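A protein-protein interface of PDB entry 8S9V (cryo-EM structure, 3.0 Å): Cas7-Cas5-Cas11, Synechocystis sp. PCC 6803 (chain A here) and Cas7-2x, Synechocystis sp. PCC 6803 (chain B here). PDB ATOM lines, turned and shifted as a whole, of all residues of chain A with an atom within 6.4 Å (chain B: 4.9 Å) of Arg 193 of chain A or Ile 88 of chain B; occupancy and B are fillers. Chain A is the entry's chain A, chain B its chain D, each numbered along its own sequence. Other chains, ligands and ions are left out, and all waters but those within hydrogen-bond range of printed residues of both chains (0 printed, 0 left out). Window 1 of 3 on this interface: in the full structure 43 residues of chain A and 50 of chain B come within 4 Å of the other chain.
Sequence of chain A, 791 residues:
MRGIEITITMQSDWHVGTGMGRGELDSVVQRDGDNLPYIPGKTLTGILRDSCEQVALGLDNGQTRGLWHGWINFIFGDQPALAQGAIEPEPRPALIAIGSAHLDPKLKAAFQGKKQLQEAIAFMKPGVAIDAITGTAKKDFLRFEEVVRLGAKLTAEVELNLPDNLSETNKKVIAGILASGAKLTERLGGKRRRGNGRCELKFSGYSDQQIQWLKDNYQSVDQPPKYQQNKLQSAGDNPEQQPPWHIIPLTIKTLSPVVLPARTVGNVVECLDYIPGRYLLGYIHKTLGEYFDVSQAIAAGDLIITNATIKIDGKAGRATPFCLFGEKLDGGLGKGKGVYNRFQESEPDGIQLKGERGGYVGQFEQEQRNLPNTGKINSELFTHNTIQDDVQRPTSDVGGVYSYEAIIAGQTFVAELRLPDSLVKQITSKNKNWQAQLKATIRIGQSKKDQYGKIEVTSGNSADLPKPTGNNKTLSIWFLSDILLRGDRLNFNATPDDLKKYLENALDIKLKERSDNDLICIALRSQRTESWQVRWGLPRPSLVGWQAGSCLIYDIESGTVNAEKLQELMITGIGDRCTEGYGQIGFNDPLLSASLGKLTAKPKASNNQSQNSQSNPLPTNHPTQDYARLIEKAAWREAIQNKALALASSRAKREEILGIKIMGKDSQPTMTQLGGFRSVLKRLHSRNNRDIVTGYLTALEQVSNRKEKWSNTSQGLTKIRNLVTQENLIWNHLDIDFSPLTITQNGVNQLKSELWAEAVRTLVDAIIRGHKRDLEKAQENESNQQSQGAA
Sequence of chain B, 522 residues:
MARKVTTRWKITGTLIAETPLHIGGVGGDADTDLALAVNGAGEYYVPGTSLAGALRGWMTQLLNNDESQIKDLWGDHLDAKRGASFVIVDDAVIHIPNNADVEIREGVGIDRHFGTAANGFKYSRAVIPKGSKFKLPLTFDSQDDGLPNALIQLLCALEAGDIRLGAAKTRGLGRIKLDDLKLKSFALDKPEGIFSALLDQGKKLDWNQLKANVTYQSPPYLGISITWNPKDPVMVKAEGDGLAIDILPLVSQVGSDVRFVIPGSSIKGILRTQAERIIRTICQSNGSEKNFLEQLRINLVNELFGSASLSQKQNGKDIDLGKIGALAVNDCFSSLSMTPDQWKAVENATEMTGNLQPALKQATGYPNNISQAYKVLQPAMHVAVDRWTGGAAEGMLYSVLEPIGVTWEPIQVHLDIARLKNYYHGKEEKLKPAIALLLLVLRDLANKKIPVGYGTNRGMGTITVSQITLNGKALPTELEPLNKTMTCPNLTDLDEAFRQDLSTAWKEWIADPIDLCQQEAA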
ATOM      1  N   ARG A 187      -3.991  -7.192 -15.131  1.00  0.00           N
ATOM      2  CA  ARG A 187      -3.465  -8.337 -14.403  1.00  0.00           C
ATOM      3  C   ARG A 187      -2.094  -8.724 -14.922  1.00  0.00           C
ATOM      4  O   ARG A 187      -1.753  -8.451 -16.070  1.00  0.00           O
ATOM      5  CB  ARG A 187      -4.408  -9.536 -14.448  1.00  0.00           C
ATOM      6  CG  ARG A 187      -5.363  -9.554 -13.284  1.00  0.00           C
ATOM      7  CD  ARG A 187      -6.474 -10.575 -13.354  1.00  0.00           C
ATOM      8  NE  ARG A 187      -7.455 -10.260 -14.356  1.00  0.00           N
ATOM      9  CZ  ARG A 187      -8.486  -9.479 -14.099  1.00  0.00           C
ATOM     10  NH1 ARG A 187      -9.262  -9.028 -15.061  1.00  0.00           N
ATOM     11  NH2 ARG A 187      -8.637  -9.030 -12.874  1.00  0.00           N
ATOM     12  N   GLY A 189       1.433 -11.684 -13.879  1.00  0.00           N
ATOM     13  CA  GLY A 189       1.977 -12.779 -13.103  1.00  0.00           C
ATOM     14  C   GLY A 189       1.191 -14.072 -13.194  1.00  0.00           C
ATOM     15  O   GLY A 189       0.413 -14.284 -14.107  1.00  0.00           O
ATOM     16  N   GLY A 190       1.400 -14.938 -12.213  1.00  0.00           N
ATOM     17  CA  GLY A 190       0.831 -16.268 -12.234  1.00  0.00           C
ATOM     18  C   GLY A 190      -0.564 -16.308 -11.667  1.00  0.00           C
ATOM     19  O   GLY A 190      -0.893 -15.565 -10.769  1.00  0.00           O
ATOM     20  N   LYS A 191      -1.389 -17.192 -12.217  1.00  0.00           N
ATOM     21  CA  LYS A 191      -2.788 -17.326 -11.813  1.00  0.00           C
ATOM     22  C   LYS A 191      -3.575 -16.041 -11.974  1.00  0.00           C
ATOM     23  O   LYS A 191      -4.449 -15.740 -11.175  1.00  0.00           O
ATOM     24  CB  LYS A 191      -2.931 -17.842 -10.392  1.00  0.00           C
ATOM     25  CG  LYS A 191      -2.268 -19.131 -10.097  1.00  0.00           C
ATOM     26  CD  LYS A 191      -2.978 -20.165 -10.932  1.00  0.00           C
ATOM     27  CE  LYS A 191      -2.220 -21.439 -11.068  1.00  0.00           C
ATOM     28  NZ  LYS A 191      -2.304 -22.158  -9.783  1.00  0.00           N
ATOM     29  N   ARG A 192      -3.279 -15.283 -13.017  1.00  0.00           N
ATOM     30  CA  ARG A 192      -4.075 -14.107 -13.317  1.00  0.00           C
ATOM     31  C   ARG A 192      -5.553 -14.429 -13.419  1.00  0.00           C
ATOM     32  O   ARG A 192      -6.398 -13.732 -12.860  1.00  0.00           O
ATOM     33  CB  ARG A 192      -3.627 -13.517 -14.629  1.00  0.00           C
ATOM     34  CG  ARG A 192      -2.437 -12.774 -14.533  1.00  0.00           C
ATOM     35  CD  ARG A 192      -2.004 -12.381 -15.873  1.00  0.00           C
ATOM     36  NE  ARG A 192      -1.176 -13.356 -16.515  1.00  0.00           N
ATOM     37  CZ  ARG A 192      -0.736 -13.186 -17.737  1.00  0.00           C
ATOM     38  NH1 ARG A 192       0.036 -14.086 -18.307  1.00  0.00           N
ATOM     39  NH2 ARG A 192      -1.085 -12.099 -18.384  1.00  0.00           N
ATOM     40  N   ARG A 193      -5.883 -15.463 -14.178  1.00  0.00           N
ATOM     41  CA  ARG A 193      -7.254 -15.866 -14.400  1.00  0.00           C
ATOM     42  C   ARG A 193      -7.963 -16.299 -13.133  1.00  0.00           C
ATOM     43  O   ARG A 193      -9.165 -16.546 -13.174  1.00  0.00           O
ATOM     44  CB  ARG A 193      -7.280 -16.980 -15.422  1.00  0.00           C
ATOM     45  CG  ARG A 193      -7.432 -16.532 -16.838  1.00  0.00           C
ATOM     46  CD  ARG A 193      -6.457 -15.499 -17.269  1.00  0.00           C
ATOM     47  NE  ARG A 193      -5.138 -16.024 -17.567  1.00  0.00           N
ATOM     48  CZ  ARG A 193      -4.431 -15.657 -18.624  1.00  0.00           C
ATOM     49  NH1 ARG A 193      -3.200 -16.078 -18.784  1.00  0.00           N
ATOM     50  NH2 ARG A 193      -4.936 -14.810 -19.485  1.00  0.00           N
ATOM     51  N   ARG A 194      -7.263 -16.422 -12.020  1.00  0.00           N
ATOM     52  CA  ARG A 194      -7.859 -16.837 -10.760  1.00  0.00           C
ATOM     53  C   ARG A 194      -7.646 -15.806  -9.665  1.00  0.00           C
ATOM     54  O   ARG A 194      -7.796 -16.110  -8.486  1.00  0.00           O
ATOM     55  CB  ARG A 194      -7.321 -18.202 -10.348  1.00  0.00           C
ATOM     56  CG  ARG A 194      -7.489 -19.299 -11.372  1.00  0.00           C
ATOM     57  CD  ARG A 194      -8.961 -19.577 -11.604  1.00  0.00           C
ATOM     58  NE  ARG A 194      -9.221 -20.501 -12.699  1.00  0.00           N
ATOM     59  CZ  ARG A 194      -9.875 -20.205 -13.812  1.00  0.00           C
ATOM     60  NH1 ARG A 194     -10.155 -21.143 -14.680  1.00  0.00           N
ATOM     61  NH2 ARG A 194     -10.326 -18.993 -14.017  1.00  0.00           N
ATOM     62  N   GLY A 195      -7.296 -14.599 -10.038  1.00  0.00           N
ATOM     63  CA  GLY A 195      -7.367 -13.455  -9.172  1.00  0.00           C
ATOM     64  C   GLY A 195      -6.055 -12.952  -8.631  1.00  0.00           C
ATOM     65  O   GLY A 195      -6.019 -11.834  -8.121  1.00  0.00           O
ATOM     66  N   ASN A 196      -4.983 -13.717  -8.718  1.00  0.00           N
ATOM     67  CA  ASN A 196      -3.676 -13.181  -8.393  1.00  0.00           C
ATOM     68  C   ASN A 196      -3.328 -12.021  -9.305  1.00  0.00           C
ATOM     69  O   ASN A 196      -3.802 -11.925 -10.430  1.00  0.00           O
ATOM     70  CB  ASN A 196      -2.610 -14.251  -8.494  1.00  0.00           C
ATOM     71  CG  ASN A 196      -2.565 -15.119  -7.292  1.00  0.00           C
ATOM     72  OD1 ASN A 196      -3.420 -15.030  -6.433  1.00  0.00           O
ATOM     73  ND2 ASN A 196      -1.563 -15.966  -7.211  1.00  0.00           N
ATOM     74  N   GLN A 392      -2.266 -18.575 -25.063  1.00  0.00           N
ATOM     75  CA  GLN A 392      -1.881 -17.781 -23.901  1.00  0.00           C
ATOM     76  C   GLN A 392      -1.044 -18.557 -22.899  1.00  0.00           C
ATOM     77  O   GLN A 392      -1.028 -18.241 -21.719  1.00  0.00           O
ATOM     78  CB  GLN A 392      -3.111 -17.202 -23.221  1.00  0.00           C
ATOM     79  CG  GLN A 392      -3.710 -16.086 -23.997  1.00  0.00           C
ATOM     80  CD  GLN A 392      -2.911 -14.857 -23.910  1.00  0.00           C
ATOM     81  OE1 GLN A 392      -2.598 -14.401 -22.831  1.00  0.00           O
ATOM     82  NE2 GLN A 392      -2.530 -14.321 -25.043  1.00  0.00           N
ATOM     83  N   ALA B  84      -5.147 -21.092 -21.785  1.00  0.00           N
ATOM     84  CA  ALA B  84      -5.642 -20.242 -20.709  1.00  0.00           C
ATOM     85  C   ALA B  84      -7.159 -20.090 -20.684  1.00  0.00           C
ATOM     86  O   ALA B  84      -7.841 -20.146 -21.704  1.00  0.00           O
ATOM     87  CB  ALA B  84      -5.011 -18.864 -20.790  1.00  0.00           C
ATOM     88  N   SER B  85      -7.668 -19.934 -19.470  1.00  0.00           N
ATOM     89  CA  SER B  85      -9.081 -19.772 -19.157  1.00  0.00           C
ATOM     90  C   SER B  85      -9.703 -18.521 -19.765  1.00  0.00           C
ATOM     91  O   SER B  85      -9.108 -17.447 -19.746  1.00  0.00           O
ATOM     92  CB  SER B  85      -9.210 -19.729 -17.647  1.00  0.00           C
ATOM     93  OG  SER B  85     -10.538 -19.693 -17.224  1.00  0.00           O
ATOM     94  N   PHE B  86     -10.912 -18.653 -20.312  1.00  0.00           N
ATOM     95  CA  PHE B  86     -11.658 -17.481 -20.773  1.00  0.00           C
ATOM     96  C   PHE B  86     -12.462 -16.792 -19.682  1.00  0.00           C
ATOM     97  O   PHE B  86     -12.683 -15.586 -19.768  1.00  0.00           O
ATOM     98  CB  PHE B  86     -12.621 -17.840 -21.894  1.00  0.00           C
ATOM     99  CG  PHE B  86     -11.954 -18.266 -23.140  1.00  0.00           C
ATOM    100  CD1 PHE B  86     -11.510 -17.330 -24.032  1.00  0.00           C
ATOM    101  CD2 PHE B  86     -11.755 -19.582 -23.420  1.00  0.00           C
ATOM    102  CE1 PHE B  86     -10.898 -17.699 -25.152  1.00  0.00           C
ATOM    103  CE2 PHE B  86     -11.133 -19.943 -24.558  1.00  0.00           C
ATOM    104  CZ  PHE B  86     -10.708 -19.002 -25.420  1.00  0.00           C
ATOM    105  N   VAL B  87     -12.932 -17.528 -18.686  1.00  0.00           N
ATOM    106  CA  VAL B  87     -13.512 -16.957 -17.479  1.00  0.00           C
ATOM    107  C   VAL B  87     -12.428 -16.570 -16.488  1.00  0.00           C
ATOM    108  O   VAL B  87     -11.605 -17.398 -16.103  1.00  0.00           O
ATOM    109  CB  VAL B  87     -14.486 -17.950 -16.854  1.00  0.00           C
ATOM    110  CG1 VAL B  87     -15.215 -17.313 -15.710  1.00  0.00           C
ATOM    111  CG2 VAL B  87     -15.437 -18.429 -17.889  1.00  0.00           C
ATOM    112  N   ILE B  88     -12.458 -15.323 -16.033  1.00  0.00           N
ATOM    113  CA  ILE B  88     -11.534 -14.799 -15.036  1.00  0.00           C
ATOM    114  C   ILE B  88     -12.304 -14.539 -13.752  1.00  0.00           C
ATOM    115  O   ILE B  88     -13.341 -13.876 -13.775  1.00  0.00           O
ATOM    116  CB  ILE B  88     -10.886 -13.505 -15.529  1.00  0.00           C
ATOM    117  CG1 ILE B  88     -10.010 -13.800 -16.719  1.00  0.00           C
ATOM    118  CG2 ILE B  88     -10.121 -12.870 -14.440  1.00  0.00           C
ATOM    119  CD1 ILE B  88     -10.020 -12.732 -17.725  1.00  0.00           C
ATOM    120  N   VAL B  89     -11.790 -15.034 -12.633  1.00  0.00           N
ATOM    121  CA  VAL B  89     -12.422 -14.865 -11.330  1.00  0.00           C
ATOM    122  C   VAL B  89     -11.425 -14.195 -10.406  1.00  0.00           C
ATOM    123  O   VAL B  89     -10.363 -14.756 -10.132  1.00  0.00           O
ATOM    124  CB  VAL B  89     -12.878 -16.203 -10.745  1.00  0.00           C
ATOM    125  CG1 VAL B  89     -13.731 -15.964  -9.572  1.00  0.00           C
ATOM    126  CG2 VAL B  89     -13.618 -17.004 -11.763  1.00  0.00           C
ATOM    127  N   ASP B  90     -11.738 -12.990  -9.958  1.00  0.00           N
ATOM    128  CA  ASP B  90     -10.895 -12.271  -9.020  1.00  0.00           C
ATOM    129  C   ASP B  90     -11.109 -12.717  -7.579  1.00  0.00           C
ATOM    130  O   ASP B  90     -12.064 -13.409  -7.244  1.00  0.00           O
ATOM    131  CB  ASP B  90     -11.133 -10.780  -9.152  1.00  0.00           C
ATOM    132  CG  ASP B  90     -10.936 -10.296 -10.553  1.00  0.00           C
ATOM    133  OD1 ASP B  90      -9.780 -10.353 -11.006  1.00  0.00           O
ATOM    134  OD2 ASP B  90     -11.908  -9.876 -11.211  1.00  0.00           O
ATOM    135  N   PRO B 137     -16.954 -11.399  -8.942  1.00  0.00           N
ATOM    136  CA  PRO B 137     -15.958 -10.689  -9.734  1.00  0.00           C
ATOM    137  C   PRO B 137     -15.574 -11.401 -11.025  1.00  0.00           C
ATOM    138  O   PRO B 137     -14.394 -11.675 -11.220  1.00  0.00           O
ATOM    139  CB  PRO B 137     -14.798 -10.616  -8.755  1.00  0.00           C
ATOM    140  CG  PRO B 137     -14.838 -11.964  -8.137  1.00  0.00           C
ATOM    141  CD  PRO B 137     -16.287 -12.433  -8.144  1.00  0.00           C
ATOM    142  N   LEU B 138     -16.522 -11.701 -11.909  1.00  0.00           N
ATOM    143  CA  LEU B 138     -16.271 -12.476 -13.120  1.00  0.00           C
ATOM    144  C   LEU B 138     -16.010 -11.571 -14.313  1.00  0.00           C
ATOM    145  O   LEU B 138     -16.583 -10.491 -14.421  1.00  0.00           O
ATOM    146  CB  LEU B 138     -17.436 -13.393 -13.458  1.00  0.00           C
ATOM    147  CG  LEU B 138     -17.905 -14.473 -12.511  1.00  0.00           C
ATOM    148  CD1 LEU B 138     -19.035 -15.224 -13.151  1.00  0.00           C
ATOM    149  CD2 LEU B 138     -16.797 -15.387 -12.202  1.00  0.00           C
ATOM    150  N   THR B 139     -15.107 -12.006 -15.180  1.00  0.00           N
ATOM    151  CA  THR B 139     -14.912 -11.466 -16.517  1.00  0.00           C
ATOM    152  C   THR B 139     -14.916 -12.623 -17.497  1.00  0.00           C
ATOM    153  O   THR B 139     -14.432 -13.700 -17.170  1.00  0.00           O
ATOM    154  CB  THR B 139     -13.580 -10.722 -16.618  1.00  0.00           C
ATOM    155  OG1 THR B 139     -13.589  -9.587 -15.751  1.00  0.00           O
ATOM    156  CG2 THR B 139     -13.322 -10.263 -18.022  1.00  0.00           C
ATOM    157  N   ASP B 141     -14.079 -13.494 -21.651  1.00  0.00           N
ATOM    158  CA  ASP B 141     -13.560 -13.049 -22.948  1.00  0.00           C
ATOM    159  C   ASP B 141     -14.121 -13.904 -24.080  1.00  0.00           C
ATOM    160  O   ASP B 141     -13.556 -14.931 -24.434  1.00  0.00           O
ATOM    161  CB  ASP B 141     -12.041 -13.115 -22.967  1.00  0.00           C
ATOM    162  CG  ASP B 141     -11.380 -12.013 -22.176  1.00  0.00           C
ATOM    163  OD1 ASP B 141     -12.065 -11.132 -21.641  1.00  0.00           O
ATOM    164  OD2 ASP B 141     -10.144 -12.039 -22.084  1.00  0.00           O
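Of the 11 printed residues of chain B, 6 touch a printed residue of chain A. Hydrophobic or aromatic side chains of chain B within 4 Å of the printed part of chain A: Ala 84 and Ile 88. Along chain A the printed residues that touch a printed residue of chain B span positions 187 to 392. Among the printed residues, Asp or Glu carboxylates within 4 Å of a Lys or Arg side-chain nitrogen of the other chain: Arg 187 of chain A with Asp 90 of chain B.
OG of Ser 85 of chain B is in hydrogen-bond range of O of Val 87 of chain B, 2.8 Å away. The backbone NH (N) of Ile 88 of chain B is in hydrogen-bond range of the backbone carbonyl oxygen (O) of Thr 139 of chain B (2.8 Å). The backbone carbonyl oxygen (O) of Pro 137 of chain B sits at hydrogen-bond distance from the backbone NH (N) of Asp 90 of chain B.
The guanidinium group of Arg 187 of chain A lies within salt-bridge range of the side-chain carboxylate of Asp 90 of chain B, at 2.6 Å. The backbone carbonyl oxygen (O) of Arg 193 of chain A lies within hydrogen-bond range of the backbone NH (N) of Val 89 of chain B, at 3.1 Å. NH1 of Arg 194 of chain A sits at hydrogen-bond distance from OG of Ser 85 of chain B. O of Val 87 of chain B lies within hydrogen-bond range of NH2 of Arg 194 of chain A. O of Val 89 of chain B lies within hydrogen-bond range of N of Gly 195 of chain A (3.1 Å). O of Arg 194 of chain A lies close to O of Val 89 of chain B, 3.3 Å away.
Arg 192 of chain A touches none of the printed residues of chain B. Of the printed residues of chain B, Arg 193 of chain A touches Ala 84 (3.9 Å), Ser 85 (3.5 Å), Val 87 (3.9 Å), Ile 88 (3.5 Å) and Val 89 (3.1 Å). Printed residues of chain B within 4 Å of Arg 194 of chain A: Ser 85 (3.0 Å), Val 87 (2.9 Å) and Val 89 (3.0 Å). Of chain A, only Arg 187 and Arg 193 come within 4 Å of Ile 88 of chain B. Of the printed residues of chain A, Val 89 of chain B touches Arg 193, Arg 194 and Gly 195. Asp 141 of chain B touches none of the printed residues of chain A. The nearest printed residue of chain A that does not touch Ser 85 of chain B is Gln 392 of chain A (6.5 Å).
Arg 187 of chain A touches Ile 88 of chain B (NE to CG2, 3.7 Å). Arg 193 of chain A touches Ala 84 of chain B (NH1 to CB, 3.9 Å). CG of Arg 193 of chain A touches O of Ser 85 of chain B, 3.5 Å away. Arg 193 of chain A touches Val 87 of chain B. CA of Ile 88 of chain B touches O of Arg 193 of chain A, 3.5 Å away. Gly 195 of chain A touches Asp 90 of chain B. Gln 392 of chain A touches Ala 84 of chain B.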
